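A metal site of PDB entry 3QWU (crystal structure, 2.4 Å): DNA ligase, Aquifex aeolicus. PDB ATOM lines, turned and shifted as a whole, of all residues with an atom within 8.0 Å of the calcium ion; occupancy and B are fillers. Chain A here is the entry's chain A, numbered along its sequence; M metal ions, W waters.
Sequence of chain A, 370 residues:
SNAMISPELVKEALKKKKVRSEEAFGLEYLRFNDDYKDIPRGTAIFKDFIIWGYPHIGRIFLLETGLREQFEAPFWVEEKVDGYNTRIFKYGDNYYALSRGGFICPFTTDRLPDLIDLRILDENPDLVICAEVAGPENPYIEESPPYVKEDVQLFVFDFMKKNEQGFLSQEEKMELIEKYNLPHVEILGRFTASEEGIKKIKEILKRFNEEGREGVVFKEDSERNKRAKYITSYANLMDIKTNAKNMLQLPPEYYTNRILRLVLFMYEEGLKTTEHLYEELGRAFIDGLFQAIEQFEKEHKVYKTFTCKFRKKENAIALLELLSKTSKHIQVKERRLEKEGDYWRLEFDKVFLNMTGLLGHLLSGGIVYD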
ATOM      1  N   LYS A  80     -18.455  36.382  -6.679  1.00  0.00           N
ATOM      2  CA  LYS A  80     -17.362  35.791  -7.400  1.00  0.00           C
ATOM      3  C   LYS A  80     -17.536  34.253  -7.307  1.00  0.00           C
ATOM      4  O   LYS A  80     -17.507  33.620  -6.232  1.00  0.00           O
ATOM      5  CB  LYS A  80     -16.002  36.259  -6.829  1.00  0.00           C
ATOM      6  CG  LYS A  80     -14.887  35.968  -7.827  1.00  0.00           C
ATOM      7  CD  LYS A  80     -13.474  36.191  -7.353  1.00  0.00           C
ATOM      8  CE  LYS A  80     -12.454  35.437  -8.337  1.00  0.00           C
ATOM      9  NZ  LYS A  80     -12.937  34.036  -8.911  1.00  0.00           N
ATOM     10  N   VAL A  81     -17.824  33.652  -8.445  1.00  0.00           N
ATOM     11  CA  VAL A  81     -18.141  32.228  -8.497  1.00  0.00           C
ATOM     12  C   VAL A  81     -16.840  31.508  -8.861  1.00  0.00           C
ATOM     13  O   VAL A  81     -16.108  31.894  -9.779  1.00  0.00           O
ATOM     14  CB  VAL A  81     -19.257  31.924  -9.548  1.00  0.00           C
ATOM     15  CG1 VAL A  81     -19.358  30.420  -9.786  1.00  0.00           C
ATOM     16  CG2 VAL A  81     -20.585  32.464  -9.103  1.00  0.00           C
ATOM     17  N   ASP A  82     -16.571  30.451  -8.124  1.00  0.00           N
ATOM     18  CA  ASP A  82     -15.345  29.714  -8.256  1.00  0.00           C
ATOM     19  C   ASP A  82     -15.518  28.603  -9.292  1.00  0.00           C
ATOM     20  O   ASP A  82     -16.002  27.521  -8.996  1.00  0.00           O
ATOM     21  CB  ASP A  82     -14.935  29.158  -6.910  1.00  0.00           C
ATOM     22  CG  ASP A  82     -13.547  28.504  -6.945  1.00  0.00           C
ATOM     23  OD1 ASP A  82     -12.726  28.800  -7.852  1.00  0.00           O
ATOM     24  OD2 ASP A  82     -13.249  27.708  -6.039  1.00  0.00           O
ATOM     25  N   GLY A  83     -15.110  28.902 -10.509  1.00  0.00           N
ATOM     26  CA  GLY A  83     -15.153  27.945 -11.610  1.00  0.00           C
ATOM     27  C   GLY A  83     -14.048  28.367 -12.560  1.00  0.00           C
ATOM     28  O   GLY A  83     -12.982  28.748 -12.123  1.00  0.00           O
ATOM     29  N   ILE A 141     -11.164  22.170 -12.770  1.00  0.00           N
ATOM     30  CA  ILE A 141     -11.178  22.608 -11.382  1.00  0.00           C
ATOM     31  C   ILE A 141     -11.898  21.498 -10.604  1.00  0.00           C
ATOM     32  O   ILE A 141     -13.022  21.126 -10.931  1.00  0.00           O
ATOM     33  CB  ILE A 141     -11.971  23.959 -11.315  1.00  0.00           C
ATOM     34  CG1 ILE A 141     -11.191  25.068 -12.038  1.00  0.00           C
ATOM     35  CG2 ILE A 141     -12.275  24.402  -9.895  1.00  0.00           C
ATOM     36  CD1 ILE A 141      -9.796  25.337 -11.450  1.00  0.00           C
ATOM     37  N   GLU A 143     -12.669  21.697  -7.401  1.00  0.00           N
ATOM     38  CA  GLU A 143     -13.662  22.385  -6.533  1.00  0.00           C
ATOM     39  C   GLU A 143     -14.952  22.758  -7.258  1.00  0.00           C
ATOM     40  O   GLU A 143     -14.947  23.034  -8.460  1.00  0.00           O
ATOM     41  CB  GLU A 143     -13.084  23.701  -5.928  1.00  0.00           C
ATOM     42  CG  GLU A 143     -12.003  23.551  -4.811  1.00  0.00           C
ATOM     43  CD  GLU A 143     -11.611  24.916  -4.166  1.00  0.00           C
ATOM     44  OE1 GLU A 143     -10.918  25.731  -4.821  1.00  0.00           O
ATOM     45  OE2 GLU A 143     -12.004  25.160  -2.977  1.00  0.00           O
ATOM     46  N   SER A 144     -16.019  22.836  -6.487  1.00  0.00           N
ATOM     47  CA  SER A 144     -17.345  23.246  -6.950  1.00  0.00           C
ATOM     48  C   SER A 144     -17.911  24.283  -5.995  1.00  0.00           C
ATOM     49  O   SER A 144     -17.625  24.212  -4.812  1.00  0.00           O
ATOM     50  CB  SER A 144     -18.283  22.038  -6.918  1.00  0.00           C
ATOM     51  OG  SER A 144     -19.461  22.276  -7.658  1.00  0.00           O
ATOM     52  N   GLY A 212     -19.545  29.218   2.521  1.00  0.00           N
ATOM     53  CA  GLY A 212     -18.543  28.623   1.608  1.00  0.00           C
ATOM     54  C   GLY A 212     -18.498  29.236   0.236  1.00  0.00           C
ATOM     55  O   GLY A 212     -18.174  28.564  -0.716  1.00  0.00           O
ATOM     56  N   ARG A 213     -18.846  30.487   0.096  1.00  0.00           N
ATOM     57  CA  ARG A 213     -18.758  31.136  -1.228  1.00  0.00           C
ATOM     58  C   ARG A 213     -17.385  31.735  -1.424  1.00  0.00           C
ATOM     59  O   ARG A 213     -16.630  31.886  -0.453  1.00  0.00           O
ATOM     60  CB  ARG A 213     -19.869  32.190  -1.345  1.00  0.00           C
ATOM     61  CG  ARG A 213     -21.183  31.462  -1.637  1.00  0.00           C
ATOM     62  CD  ARG A 213     -22.391  32.248  -1.700  1.00  0.00           C
ATOM     63  NE  ARG A 213     -23.480  31.285  -1.742  1.00  0.00           N
ATOM     64  CZ  ARG A 213     -24.330  31.123  -2.758  1.00  0.00           C
ATOM     65  NH1 ARG A 213     -24.313  31.922  -3.853  1.00  0.00           N
ATOM     66  NH2 ARG A 213     -25.245  30.170  -2.627  1.00  0.00           N
ATOM     67  N   GLU A 214     -17.020  32.013  -2.664  1.00  0.00           N
ATOM     68  CA  GLU A 214     -15.636  32.409  -2.893  1.00  0.00           C
ATOM     69  C   GLU A 214     -15.319  33.826  -2.432  1.00  0.00           C
ATOM     70  O   GLU A 214     -14.253  34.082  -1.870  1.00  0.00           O
ATOM     71  CB  GLU A 214     -15.226  32.242  -4.334  1.00  0.00           C
ATOM     72  CG  GLU A 214     -13.722  32.427  -4.465  1.00  0.00           C
ATOM     73  CD  GLU A 214     -13.240  32.143  -5.867  1.00  0.00           C
ATOM     74  OE1 GLU A 214     -12.221  31.417  -5.984  1.00  0.00           O
ATOM     75  OE2 GLU A 214     -13.886  32.603  -6.844  1.00  0.00           O
ATOM     76  N   ILE A 231     -11.645  37.972  -1.469  1.00  0.00           N
ATOM     77  CA  ILE A 231     -11.842  36.517  -1.272  1.00  0.00           C
ATOM     78  C   ILE A 231     -12.110  36.218   0.224  1.00  0.00           C
ATOM     79  O   ILE A 231     -11.549  36.845   1.119  1.00  0.00           O
ATOM     80  CB  ILE A 231     -10.589  35.747  -1.782  1.00  0.00           C
ATOM     81  CG1 ILE A 231     -10.165  36.350  -3.161  1.00  0.00           C
ATOM     82  CG2 ILE A 231     -10.797  34.197  -1.895  1.00  0.00           C
ATOM     83  CD1 ILE A 231     -10.970  36.000  -4.519  1.00  0.00           C
ATOM     84  N   THR A 232     -12.987  35.267   0.483  1.00  0.00           N
ATOM     85  CA  THR A 232     -13.250  34.835   1.851  1.00  0.00           C
ATOM     86  C   THR A 232     -12.078  34.022   2.388  1.00  0.00           C
ATOM     87  O   THR A 232     -11.297  33.457   1.623  1.00  0.00           O
ATOM     88  CB  THR A 232     -14.515  34.004   1.931  1.00  0.00           C
ATOM     89  OG1 THR A 232     -14.376  32.831   1.093  1.00  0.00           O
ATOM     90  CG2 THR A 232     -15.762  34.853   1.497  1.00  0.00           C
ATOM     91  N   TYR A 234     -12.379  31.322   4.068  1.00  0.00           N
ATOM     92  CA  TYR A 234     -12.717  29.950   3.677  1.00  0.00           C
ATOM     93  C   TYR A 234     -12.158  29.558   2.306  1.00  0.00           C
ATOM     94  O   TYR A 234     -11.528  28.498   2.147  1.00  0.00           O
ATOM     95  CB  TYR A 234     -14.218  29.725   3.680  1.00  0.00           C
ATOM     96  CG  TYR A 234     -14.668  28.431   3.014  1.00  0.00           C
ATOM     97  CD1 TYR A 234     -14.793  28.360   1.588  1.00  0.00           C
ATOM     98  CD2 TYR A 234     -14.973  27.291   3.767  1.00  0.00           C
ATOM     99  CE1 TYR A 234     -15.216  27.197   0.983  1.00  0.00           C
ATOM    100  CE2 TYR A 234     -15.387  26.107   3.159  1.00  0.00           C
ATOM    101  CZ  TYR A 234     -15.506  26.081   1.787  1.00  0.00           C
ATOM    102  OH  TYR A 234     -15.938  24.926   1.174  1.00  0.00           O
ATOM    103  N   ALA A 235     -12.373  30.394   1.306  1.00  0.00           N
ATOM    104  CA  ALA A 235     -11.894  30.045  -0.021  1.00  0.00           C
ATOM    105  C   ALA A 235     -10.398  30.082  -0.073  1.00  0.00           C
ATOM    106  O   ALA A 235      -9.791  29.304  -0.779  1.00  0.00           O
ATOM    107  CB  ALA A 235     -12.477  30.974  -1.056  1.00  0.00           C
ATOM    108  N   ASN A 236      -9.779  31.033   0.589  1.00  0.00           N
ATOM    109  CA  ASN A 236      -8.335  31.087   0.636  1.00  0.00           C
ATOM    110  C   ASN A 236      -7.753  29.824   1.264  1.00  0.00           C
ATOM    111  O   ASN A 236      -6.890  29.197   0.678  1.00  0.00           O
ATOM    112  CB  ASN A 236      -7.852  32.340   1.421  1.00  0.00           C
ATOM    113  CG  ASN A 236      -7.962  33.606   0.612  1.00  0.00           C
ATOM    114  OD1 ASN A 236      -7.560  33.635  -0.562  1.00  0.00           O
ATOM    115  ND2 ASN A 236      -8.455  34.674   1.221  1.00  0.00           N
ATOM    116  N   LEU A 237      -8.305  29.418   2.404  1.00  0.00           N
ATOM    117  CA  LEU A 237      -7.918  28.156   3.003  1.00  0.00           C
ATOM    118  C   LEU A 237      -8.047  26.942   2.034  1.00  0.00           C
ATOM    119  O   LEU A 237      -7.114  26.181   1.856  1.00  0.00           O
ATOM    120  CB  LEU A 237      -8.713  27.930   4.279  1.00  0.00           C
ATOM    121  CG  LEU A 237      -8.306  28.834   5.420  1.00  0.00           C
ATOM    122  CD1 LEU A 237      -9.373  28.773   6.522  1.00  0.00           C
ATOM    123  CD2 LEU A 237      -6.911  28.474   5.926  1.00  0.00           C
ATOM    124  N   MET A 238      -9.220  26.798   1.428  1.00  0.00           N
ATOM    125  CA  MET A 238      -9.532  25.687   0.551  1.00  0.00           C
ATOM    126  C   MET A 238      -8.566  25.679  -0.661  1.00  0.00           C
ATOM    127  O   MET A 238      -8.188  24.640  -1.134  1.00  0.00           O
ATOM    128  CB  MET A 238     -10.964  25.816   0.001  1.00  0.00           C
ATOM    129  CG  MET A 238     -12.039  24.987   0.567  1.00  0.00           C
ATOM    130  SD  MET A 238     -11.696  23.238   1.052  1.00  0.00           S
ATOM    131  CE  MET A 238     -11.224  23.537   2.794  1.00  0.00           C
ATOM    132  N   ASP A 239      -8.205  26.854  -1.162  1.00  0.00           N
ATOM    133  CA  ASP A 239      -7.196  26.875  -2.230  1.00  0.00           C
ATOM    134  C   ASP A 239      -5.906  26.257  -1.760  1.00  0.00           C
ATOM    135  O   ASP A 239      -5.323  25.478  -2.501  1.00  0.00           O
ATOM    136  CB  ASP A 239      -6.916  28.257  -2.778  1.00  0.00           C
ATOM    137  CG  ASP A 239      -8.052  28.784  -3.627  1.00  0.00           C
ATOM    138  OD1 ASP A 239      -8.927  27.993  -4.054  1.00  0.00           O
ATOM    139  OD2 ASP A 239      -8.066  29.991  -3.851  1.00  0.00           O
ATOM    140  N   ILE A 240      -5.469  26.566  -0.528  1.00  0.00           N
ATOM    141  CA  ILE A 240      -4.205  26.039  -0.093  1.00  0.00           C
ATOM    142  C   ILE A 240      -4.328  24.525  -0.052  1.00  0.00           C
ATOM    143  O   ILE A 240      -3.528  23.817  -0.644  1.00  0.00           O
ATOM    144  CB  ILE A 240      -3.748  26.644   1.241  1.00  0.00           C
ATOM    145  CG1 ILE A 240      -3.572  28.127   1.088  1.00  0.00           C
ATOM    146  CG2 ILE A 240      -2.447  26.020   1.640  1.00  0.00           C
ATOM    147  CD1 ILE A 240      -3.132  28.841   2.324  1.00  0.00           C
ATOM    148  N   THR A 242      -6.586  22.316  -1.519  1.00  0.00           N
ATOM    149  CA  THR A 242      -6.807  21.569  -2.742  1.00  0.00           C
ATOM    150  C   THR A 242      -5.636  21.696  -3.660  1.00  0.00           C
ATOM    151  O   THR A 242      -5.573  20.993  -4.615  1.00  0.00           O
ATOM    152  CB  THR A 242      -8.059  22.032  -3.497  1.00  0.00           C
ATOM    153  OG1 THR A 242      -7.880  23.389  -3.794  1.00  0.00           O
ATOM    154  CG2 THR A 242      -9.336  21.861  -2.629  1.00  0.00           C
ATOM    155  N   ASN A 243      -4.688  22.581  -3.398  1.00  0.00           N
ATOM    156  CA  ASN A 243      -3.494  22.690  -4.226  1.00  0.00           C
ATOM    157  C   ASN A 243      -2.273  21.940  -3.706  1.00  0.00           C
ATOM    158  O   ASN A 243      -1.151  22.143  -4.189  1.00  0.00           O
ATOM    159  CB  ASN A 243      -3.133  24.143  -4.423  1.00  0.00           C
ATOM    160  CG  ASN A 243      -3.655  24.650  -5.701  1.00  0.00           C
ATOM    161  OD1 ASN A 243      -2.909  24.708  -6.701  1.00  0.00           O
ATOM    162  ND2 ASN A 243      -4.977  24.953  -5.738  1.00  0.00           N
ATOM    163  N   TYR A 254       3.029  32.121  -3.995  1.00  0.00           N
ATOM    164  CA  TYR A 254       1.802  31.538  -3.408  1.00  0.00           C
ATOM    165  C   TYR A 254       1.838  31.733  -1.848  1.00  0.00           C
ATOM    166  O   TYR A 254       0.805  32.003  -1.249  1.00  0.00           O
ATOM    167  CB  TYR A 254       1.603  30.047  -3.806  1.00  0.00           C
ATOM    168  CG  TYR A 254       0.226  29.649  -4.334  1.00  0.00           C
ATOM    169  CD1 TYR A 254      -0.197  30.007  -5.639  1.00  0.00           C
ATOM    170  CD2 TYR A 254      -0.649  28.868  -3.577  1.00  0.00           C
ATOM    171  CE1 TYR A 254      -1.497  29.622  -6.152  1.00  0.00           C
ATOM    172  CE2 TYR A 254      -1.934  28.491  -4.064  1.00  0.00           C
ATOM    173  CZ  TYR A 254      -2.364  28.862  -5.350  1.00  0.00           C
ATOM    174  OH  TYR A 254      -3.635  28.459  -5.780  1.00  0.00           O
ATOM    175  N   ARG A 258      -1.224  34.084  -0.365  1.00  0.00           N
ATOM    176  CA  ARG A 258      -2.446  33.539   0.249  1.00  0.00           C
ATOM    177  C   ARG A 258      -2.464  33.620   1.788  1.00  0.00           C
ATOM    178  O   ARG A 258      -3.513  33.777   2.400  1.00  0.00           O
ATOM    179  CB  ARG A 258      -2.759  32.162  -0.309  1.00  0.00           C
ATOM    180  CG  ARG A 258      -3.717  32.228  -1.535  1.00  0.00           C
ATOM    181  CD  ARG A 258      -3.767  30.971  -2.330  1.00  0.00           C
ATOM    182  NE  ARG A 258      -4.436  31.168  -3.622  1.00  0.00           N
ATOM    183  CZ  ARG A 258      -3.869  31.672  -4.707  1.00  0.00           C
ATOM    184  NH1 ARG A 258      -2.582  32.032  -4.733  1.00  0.00           N
ATOM    185  NH2 ARG A 258      -4.620  31.825  -5.795  1.00  0.00           N
HETATM  186 CA    CA M   1     -11.454  28.147  -4.221  1.00  0.00          CA
HETATM  187  O   HOH W   1     -10.433  28.337  -6.334  1.00  0.00           O
HETATM  188  O   HOH W   2     -10.495  30.159  -4.447  1.00  0.00           O
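OE2 of Glu 214 is in salt-bridge range of NZ of Lys 80, 2.7 Å away. The backbone carbonyl oxygen (O) of Asp 239 sits close to the side-chain amide nitrogen (ND2) of Asn 243 (3.3 Å). The side-chain carboxylate (OD2) of Asp 239 is in salt-bridge range of the guanidinium group (NE) of Arg 258 (3.8 Å). The backbone NH of Ala 235 sits at hydrogen-bond distance from the side-chain hydroxyl of Thr 232, 3.2 Å away. O of Glu 214 lies within hydrogen-bond range of N of Thr 232, 2.9 Å away.
Glu 214 touches the calcium ion (OE1 to CA, 3.8 Å). Ala 235 touches the calcium ion (O to CA, 3.99 Å). Of the 23 residues printed, 5 come within 4 Å of the calcium ion.
Water W2 binds the calcium ion, 2.2 Å away. Water W1 binds the calcium ion (2.4 Å). OD1 of Asp 239 is bound to the calcium ion (2.5 Å). OE1 of Glu 143 binds the calcium ion. The calcium ion is bound by the side-chain carboxylate (OD2) of Asp 82 (2.6 Å).
Water W2 lies within hydrogen-bond range of OD2 of Asp 239 (2.5 Å) and OE1 of Glu 214 (2.6 Å).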
